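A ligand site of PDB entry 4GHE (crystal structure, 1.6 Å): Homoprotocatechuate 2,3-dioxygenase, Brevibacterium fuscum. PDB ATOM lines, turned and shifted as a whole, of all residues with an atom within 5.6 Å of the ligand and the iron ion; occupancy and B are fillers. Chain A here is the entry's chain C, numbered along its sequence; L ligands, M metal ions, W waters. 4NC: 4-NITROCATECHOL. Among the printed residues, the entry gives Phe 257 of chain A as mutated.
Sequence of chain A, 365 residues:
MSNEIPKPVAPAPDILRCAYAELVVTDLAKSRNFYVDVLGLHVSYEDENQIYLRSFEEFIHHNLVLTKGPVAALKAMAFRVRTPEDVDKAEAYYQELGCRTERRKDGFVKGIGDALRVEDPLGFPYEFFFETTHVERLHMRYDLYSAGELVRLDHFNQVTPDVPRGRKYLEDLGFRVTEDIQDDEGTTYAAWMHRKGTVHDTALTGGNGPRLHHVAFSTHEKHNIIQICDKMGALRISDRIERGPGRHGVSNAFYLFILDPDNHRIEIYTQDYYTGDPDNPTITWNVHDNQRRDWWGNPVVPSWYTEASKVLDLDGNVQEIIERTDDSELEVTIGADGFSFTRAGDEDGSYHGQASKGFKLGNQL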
ATOM      1  N   HIS A 155      25.156  13.827 -18.579  1.00  0.00           N
ATOM      2  CA  HIS A 155      24.120  12.806 -18.811  1.00  0.00           C
ATOM      3  C   HIS A 155      24.421  11.489 -18.219  1.00  0.00           C
ATOM      4  O   HIS A 155      25.563  11.224 -17.777  1.00  0.00           O
ATOM      5  CB  HIS A 155      23.887  12.653 -20.317  1.00  0.00           C
ATOM      6  CG  HIS A 155      25.061  12.127 -21.072  1.00  0.00           C
ATOM      7  ND1 HIS A 155      25.931  12.934 -21.758  1.00  0.00           N
ATOM      8  CD2 HIS A 155      25.448  10.845 -21.311  1.00  0.00           C
ATOM      9  CE1 HIS A 155      26.835  12.152 -22.372  1.00  0.00           C
ATOM     10  NE2 HIS A 155      26.553  10.885 -22.094  1.00  0.00           N
ATOM     11  N   ASN A 157      23.734   7.150 -19.183  1.00  0.00           N
ATOM     12  CA  ASN A 157      23.383   6.237 -20.250  1.00  0.00           C
ATOM     13  C   ASN A 157      23.044   4.902 -19.591  1.00  0.00           C
ATOM     14  O   ASN A 157      23.855   4.353 -18.839  1.00  0.00           O
ATOM     15  CB  ASN A 157      24.495   6.127 -21.288  1.00  0.00           C
ATOM     16  CG  ASN A 157      24.127   5.248 -22.452  1.00  0.00           C
ATOM     17  OD1 ASN A 157      23.750   4.090 -22.249  1.00  0.00           O
ATOM     18  ND2 ASN A 157      24.263   5.770 -23.700  1.00  0.00           N
ATOM     19  N   TRP A 192      18.719   8.714 -27.665  1.00  0.00           N
ATOM     20  CA  TRP A 192      19.246   9.757 -26.790  1.00  0.00           C
ATOM     21  C   TRP A 192      18.144  10.747 -26.576  1.00  0.00           C
ATOM     22  O   TRP A 192      17.424  11.041 -27.502  1.00  0.00           O
ATOM     23  CB  TRP A 192      20.388  10.482 -27.518  1.00  0.00           C
ATOM     24  CG  TRP A 192      21.680   9.682 -27.488  1.00  0.00           C
ATOM     25  CD1 TRP A 192      22.764   9.867 -26.655  1.00  0.00           C
ATOM     26  CD2 TRP A 192      22.057   8.545 -28.327  1.00  0.00           C
ATOM     27  NE1 TRP A 192      23.764   8.967 -26.908  1.00  0.00           N
ATOM     28  CE2 TRP A 192      23.395   8.132 -27.898  1.00  0.00           C
ATOM     29  CE3 TRP A 192      21.430   7.857 -29.331  1.00  0.00           C
ATOM     30  CZ2 TRP A 192      24.063   7.068 -28.487  1.00  0.00           C
ATOM     31  CZ3 TRP A 192      22.107   6.796 -29.920  1.00  0.00           C
ATOM     32  CH2 TRP A 192      23.388   6.400 -29.504  1.00  0.00           C
ATOM     33  N   HIS A 200      21.375  15.080 -24.726  1.00  0.00           N
ATOM     34  CA  HIS A 200      20.686  14.200 -23.776  1.00  0.00           C
ATOM     35  C   HIS A 200      20.909  14.486 -22.320  1.00  0.00           C
ATOM     36  O   HIS A 200      21.861  15.167 -21.961  1.00  0.00           O
ATOM     37  CB  HIS A 200      20.977  12.737 -24.082  1.00  0.00           C
ATOM     38  CG  HIS A 200      22.422  12.351 -24.126  1.00  0.00           C
ATOM     39  ND1 HIS A 200      23.390  13.074 -24.717  1.00  0.00           N
ATOM     40  CD2 HIS A 200      23.043  11.196 -23.654  1.00  0.00           C
ATOM     41  CE1 HIS A 200      24.550  12.389 -24.687  1.00  0.00           C
ATOM     42  NE2 HIS A 200      24.327  11.247 -24.032  1.00  0.00           N
ATOM     43  N   HIS A 214      27.089   4.295 -18.416  1.00  0.00           N
ATOM     44  CA  HIS A 214      28.027   5.331 -17.987  1.00  0.00           C
ATOM     45  C   HIS A 214      27.398   6.564 -17.405  1.00  0.00           C
ATOM     46  O   HIS A 214      26.204   6.825 -17.572  1.00  0.00           O
ATOM     47  CB  HIS A 214      29.017   5.702 -19.118  1.00  0.00           C
ATOM     48  CG  HIS A 214      28.390   6.328 -20.320  1.00  0.00           C
ATOM     49  ND1 HIS A 214      28.057   5.620 -21.400  1.00  0.00           N
ATOM     50  CD2 HIS A 214      28.153   7.636 -20.614  1.00  0.00           C
ATOM     51  CE1 HIS A 214      27.573   6.482 -22.351  1.00  0.00           C
ATOM     52  NE2 HIS A 214      27.606   7.700 -21.853  1.00  0.00           N
ATOM     53  N   ALA A 216      28.350  10.728 -17.607  1.00  0.00           N
ATOM     54  CA  ALA A 216      29.164  11.660 -18.403  1.00  0.00           C
ATOM     55  C   ALA A 216      29.311  13.032 -17.812  1.00  0.00           C
ATOM     56  O   ALA A 216      28.312  13.655 -17.438  1.00  0.00           O
ATOM     57  CB  ALA A 216      28.570  11.793 -19.809  1.00  0.00           C
ATOM     58  N   ARG A 243      38.031   3.540 -24.485  1.00  0.00           N
ATOM     59  CA  ARG A 243      37.632   3.906 -25.843  1.00  0.00           C
ATOM     60  C   ARG A 243      37.790   5.374 -25.995  1.00  0.00           C
ATOM     61  O   ARG A 243      37.351   6.124 -25.156  1.00  0.00           O
ATOM     62  CB  ARG A 243      36.174   3.560 -26.047  1.00  0.00           C
ATOM     63  CG  ARG A 243      35.624   3.938 -27.403  1.00  0.00           C
ATOM     64  CD  ARG A 243      34.273   3.348 -27.738  1.00  0.00           C
ATOM     65  NE  ARG A 243      33.789   4.195 -28.802  1.00  0.00           N
ATOM     66  CZ  ARG A 243      32.550   4.649 -28.928  1.00  0.00           C
ATOM     67  NH1 ARG A 243      31.577   4.205 -28.123  1.00  0.00           N
ATOM     68  NH2 ARG A 243      32.267   5.539 -29.860  1.00  0.00           N
ATOM     69  N   HIS A 248      32.164  11.752 -31.649  1.00  0.00           N
ATOM     70  CA  HIS A 248      30.978  10.900 -31.873  1.00  0.00           C
ATOM     71  C   HIS A 248      30.304  11.297 -33.177  1.00  0.00           C
ATOM     72  O   HIS A 248      30.337  12.473 -33.601  1.00  0.00           O
ATOM     73  CB  HIS A 248      29.924  11.148 -30.781  1.00  0.00           C
ATOM     74  CG  HIS A 248      30.208  10.524 -29.456  1.00  0.00           C
ATOM     75  ND1 HIS A 248      30.509   9.201 -29.326  1.00  0.00           N
ATOM     76  CD2 HIS A 248      30.147  11.053 -28.139  1.00  0.00           C
ATOM     77  CE1 HIS A 248      30.626   8.897 -28.004  1.00  0.00           C
ATOM     78  NE2 HIS A 248      30.421  10.043 -27.295  1.00  0.00           N
ATOM     79  N   GLY A 249      29.628  10.355 -33.816  1.00  0.00           N
ATOM     80  CA  GLY A 249      28.656  10.696 -34.859  1.00  0.00           C
ATOM     81  C   GLY A 249      27.398  11.234 -34.204  1.00  0.00           C
ATOM     82  O   GLY A 249      27.119  12.449 -34.242  1.00  0.00           O
ATOM     83  N   VAL A 250      26.625  10.330 -33.586  1.00  0.00           N
ATOM     84  CA  VAL A 250      25.522  10.723 -32.705  1.00  0.00           C
ATOM     85  C   VAL A 250      26.043  11.736 -31.700  1.00  0.00           C
ATOM     86  O   VAL A 250      26.983  11.440 -30.985  1.00  0.00           O
ATOM     87  CB  VAL A 250      24.959   9.510 -31.933  1.00  0.00           C
ATOM     88  CG1 VAL A 250      23.955   9.964 -30.872  1.00  0.00           C
ATOM     89  CG2 VAL A 250      24.383   8.469 -32.897  1.00  0.00           C
ATOM     90  N   SER A 251      25.416  12.903 -31.638  1.00  0.00           N
ATOM     91  CA  SER A 251      25.714  13.994 -30.693  1.00  0.00           C
ATOM     92  C   SER A 251      26.745  14.929 -31.188  1.00  0.00           C
ATOM     93  O   SER A 251      26.799  16.020 -30.689  1.00  0.00           O
ATOM     94  CB  SER A 251      26.067  13.532 -29.272  1.00  0.00           C
ATOM     95  OG  SER A 251      27.468  13.258 -29.145  1.00  0.00           O
ATOM     96  N   PHE A 257      36.044   7.556 -23.050  1.00  0.00           N
ATOM     97  CA  PHE A 257      35.525   6.629 -22.018  1.00  0.00           C
ATOM     98  C   PHE A 257      36.639   6.013 -21.201  1.00  0.00           C
ATOM     99  O   PHE A 257      37.582   5.455 -21.742  1.00  0.00           O
ATOM    100  CB  PHE A 257      34.710   5.505 -22.678  1.00  0.00           C
ATOM    101  CG  PHE A 257      33.458   5.975 -23.349  1.00  0.00           C
ATOM    102  CD1 PHE A 257      32.277   6.173 -22.625  1.00  0.00           C
ATOM    103  CD2 PHE A 257      33.467   6.249 -24.695  1.00  0.00           C
ATOM    104  CE1 PHE A 257      31.119   6.610 -23.264  1.00  0.00           C
ATOM    105  CE2 PHE A 257      32.302   6.646 -25.337  1.00  0.00           C
ATOM    106  CZ  PHE A 257      31.145   6.867 -24.614  1.00  0.00           C
ATOM    107  N   GLU A 267      32.204   8.787 -18.984  1.00  0.00           N
ATOM    108  CA  GLU A 267      32.451   9.480 -20.226  1.00  0.00           C
ATOM    109  C   GLU A 267      32.856  10.937 -19.916  1.00  0.00           C
ATOM    110  O   GLU A 267      32.262  11.615 -19.075  1.00  0.00           O
ATOM    111  CB  GLU A 267      31.209   9.468 -21.125  1.00  0.00           C
ATOM    112  CG  GLU A 267      31.498  10.052 -22.509  1.00  0.00           C
ATOM    113  CD  GLU A 267      30.290  10.064 -23.422  1.00  0.00           C
ATOM    114  OE1 GLU A 267      29.183   9.934 -22.873  1.00  0.00           O
ATOM    115  OE2 GLU A 267      30.520  10.164 -24.641  1.00  0.00           O
ATOM    116  N   TYR A 269      33.123  14.502 -22.162  1.00  0.00           N
ATOM    117  CA  TYR A 269      32.288  14.852 -23.302  1.00  0.00           C
ATOM    118  C   TYR A 269      32.366  16.374 -23.473  1.00  0.00           C
ATOM    119  O   TYR A 269      32.439  17.115 -22.480  1.00  0.00           O
ATOM    120  CB  TYR A 269      30.868  14.444 -22.912  1.00  0.00           C
ATOM    121  CG  TYR A 269      29.698  14.600 -23.851  1.00  0.00           C
ATOM    122  CD1 TYR A 269      29.281  13.534 -24.651  1.00  0.00           C
ATOM    123  CD2 TYR A 269      28.881  15.741 -23.809  1.00  0.00           C
ATOM    124  CE1 TYR A 269      28.139  13.654 -25.470  1.00  0.00           C
ATOM    125  CE2 TYR A 269      27.768  15.840 -24.638  1.00  0.00           C
ATOM    126  CZ  TYR A 269      27.377  14.786 -25.408  1.00  0.00           C
ATOM    127  OH  TYR A 269      26.238  14.925 -26.200  1.00  0.00           O
ATOM    128  N   ARG A 292      28.781   6.359 -37.109  1.00  0.00           N
ATOM    129  CA  ARG A 292      27.680   6.741 -36.198  1.00  0.00           C
ATOM    130  C   ARG A 292      28.130   6.882 -34.745  1.00  0.00           C
ATOM    131  O   ARG A 292      27.560   7.655 -33.991  1.00  0.00           O
ATOM    132  CB  ARG A 292      26.558   5.678 -36.303  1.00  0.00           C
ATOM    133  CG  ARG A 292      26.876   4.384 -35.570  1.00  0.00           C
ATOM    134  CD  ARG A 292      25.999   3.184 -35.906  1.00  0.00           C
ATOM    135  NE  ARG A 292      26.423   2.097 -35.051  1.00  0.00           N
ATOM    136  CZ  ARG A 292      27.528   1.382 -35.236  1.00  0.00           C
ATOM    137  NH1 ARG A 292      28.290   1.575 -36.302  1.00  0.00           N
ATOM    138  NH2 ARG A 292      27.860   0.416 -34.371  1.00  0.00           N
ATOM    139  N   ARG A 293      29.137   6.100 -34.325  1.00  0.00           N
ATOM    140  CA  ARG A 293      29.579   6.107 -32.910  1.00  0.00           C
ATOM    141  C   ARG A 293      30.889   6.850 -32.793  1.00  0.00           C
ATOM    142  O   ARG A 293      31.027   7.739 -31.968  1.00  0.00           O
ATOM    143  CB  ARG A 293      29.641   4.687 -32.347  1.00  0.00           C
ATOM    144  CG  ARG A 293      28.242   4.184 -31.996  1.00  0.00           C
ATOM    145  CD  ARG A 293      28.267   3.023 -31.063  1.00  0.00           C
ATOM    146  NE  ARG A 293      26.923   2.604 -30.659  1.00  0.00           N
ATOM    147  CZ  ARG A 293      26.142   3.164 -29.742  1.00  0.00           C
ATOM    148  NH1 ARG A 293      26.473   4.250 -29.036  1.00  0.00           N
ATOM    149  NH2 ARG A 293      24.972   2.592 -29.516  1.00  0.00           N
ATOM    150  N   ASP A 294      31.849   6.471 -33.622  1.00  0.00           N
ATOM    151  CA  ASP A 294      33.048   7.239 -33.795  1.00  0.00           C
ATOM    152  C   ASP A 294      33.044   7.759 -35.231  1.00  0.00           C
ATOM    153  O   ASP A 294      33.142   7.009 -36.202  1.00  0.00           O
ATOM    154  CB  ASP A 294      34.300   6.403 -33.529  1.00  0.00           C
ATOM    155  CG  ASP A 294      35.541   7.271 -33.494  1.00  0.00           C
ATOM    156  OD1 ASP A 294      35.820   7.856 -32.421  1.00  0.00           O
ATOM    157  OD2 ASP A 294      36.238   7.370 -34.542  1.00  0.00           O
ATOM    158  N   TRP A 304      32.827  -2.257 -24.661  1.00  0.00           N
ATOM    159  CA  TRP A 304      31.947  -1.088 -24.597  1.00  0.00           C
ATOM    160  C   TRP A 304      30.496  -1.493 -24.759  1.00  0.00           C
ATOM    161  O   TRP A 304      29.615  -0.906 -24.145  1.00  0.00           O
ATOM    162  CB  TRP A 304      32.377  -0.074 -25.659  1.00  0.00           C
ATOM    163  CG  TRP A 304      31.740   1.266 -25.452  1.00  0.00           C
ATOM    164  CD1 TRP A 304      32.248   2.318 -24.693  1.00  0.00           C
ATOM    165  CD2 TRP A 304      30.411   1.716 -25.905  1.00  0.00           C
ATOM    166  NE1 TRP A 304      31.368   3.366 -24.696  1.00  0.00           N
ATOM    167  CE2 TRP A 304      30.252   3.069 -25.392  1.00  0.00           C
ATOM    168  CE3 TRP A 304      29.358   1.136 -26.625  1.00  0.00           C
ATOM    169  CZ2 TRP A 304      29.087   3.826 -25.608  1.00  0.00           C
ATOM    170  CZ3 TRP A 304      28.201   1.901 -26.862  1.00  0.00           C
ATOM    171  CH2 TRP A 304      28.078   3.212 -26.363  1.00  0.00           C
HETATM  172  C1  4NC L   1      27.285   9.724 -26.154  1.00  0.00           C
HETATM  173  C2  4NC L   1      27.723   8.336 -26.000  1.00  0.00           C
HETATM  174  C3  4NC L   1      27.789   7.505 -27.115  1.00  0.00           C
HETATM  175  C4  4NC L   1      27.540   8.049 -28.394  1.00  0.00           C
HETATM  176  C5  4NC L   1      27.175   9.377 -28.557  1.00  0.00           C
HETATM  177  C6  4NC L   1      27.032  10.214 -27.435  1.00  0.00           C
HETATM  178  O7  4NC L   1      27.190  10.550 -25.062  1.00  0.00           O
HETATM  179  O8  4NC L   1      27.931   7.799 -24.796  1.00  0.00           O
HETATM  180  N9  4NC L   1      27.885   7.262 -29.457  1.00  0.00           N
HETATM  181  O10 4NC L   1      28.914   6.086 -29.252  1.00  0.00           O
HETATM  182  O11 4NC L   1      27.891   7.887 -30.689  1.00  0.00           O
HETATM  183 FE    FE M   1      27.369   9.235 -23.375  1.00  0.00          FE
HETATM  184  O   HOH W   1      25.159   8.599 -23.963  1.00  0.00           O
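Water W1 lies within hydrogen-bond range of a ring nitrogen (NE2) of His 200 (2.8 Å), the side-chain amide nitrogen (ND2) of Asn 157 (3.0 Å) and the indole nitrogen (NE1) of Trp 192 (3.3 Å).
O11 of the ligand sits close to O of Arg 292 (3.3 Å).
NE1 of Trp 192 touches C6 of the ligand, at 3.5 Å.
Val 250 touches the ligand (O to C5, 3.2 Å).
OG of Ser 251 touches C6 of the ligand (3.5 Å).
CZ of Phe 257 touches O8 of the ligand, 3.4 Å away.
CE1 of Tyr 269 touches O7 of the ligand, 3.3 Å away.
Of the 18 residues printed, 13 come within 4 Å of the ligand.
The nearest printed residue that does not touch the ligand is Trp 304 (4.2 Å).
OE2 of Glu 267 lies within hydrogen-bond range of NE2 of His 248.
The backbone carbonyl oxygen (O) of His 214 sits at hydrogen-bond distance from the backbone NH (N) of Asn 157, 3.0 Å away.
NE2 of His 200 sits close to ND1 of His 155 (3.3 Å).
The backbone carbonyl oxygen of His 155 sits at hydrogen-bond distance from the backbone NH of Ala 216 (2.8 Å).
A ring nitrogen (ND1) of His 248 sits at hydrogen-bond distance from the backbone carbonyl oxygen (O) of Arg 293 (3.1 Å).
O of Arg 293 is in hydrogen-bond range of NH2 of Arg 243.
The backbone NH (N) of Gly 249 lies within hydrogen-bond range of the backbone carbonyl oxygen (O) of Arg 293.
The backbone NH of Val 250 sits at hydrogen-bond distance from the backbone carbonyl oxygen of Arg 292.
Merely in contact with the iron ion: His 200.
Within 4 Å of the iron ion: His 155, His 200, His 214 and Glu 267.
The nearest printed residue that does not touch the iron ion is Ala 216 (4.5 Å).
The guanidinium group (NH1) of Arg 293 lies within hydrogen-bond range of an oxygen (O10) of the ligand (3.1 Å).
NE2 of His 200 sits close to O7 of the ligand, at 3.1 Å.
O11 of the ligand is in hydrogen-bond range of ND1 of His 248 (3.2 Å).
NH1 of Arg 243 lies within hydrogen-bond range of O10 of the ligand, at 3.5 Å.
The iron ion is bound by OE1 of Glu 267 (2.0 Å).
An oxygen (O8) of the ligand binds the iron ion (2.1 Å).
O7 of the ligand is bound to the iron ion (2.1 Å).
The iron ion is bound by a ring nitrogen (NE2) of His 214 (2.2 Å).
A ring nitrogen (NE2) of His 155 binds the iron ion (2.2 Å).
Water W1 binds the iron ion (2.4 Å).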
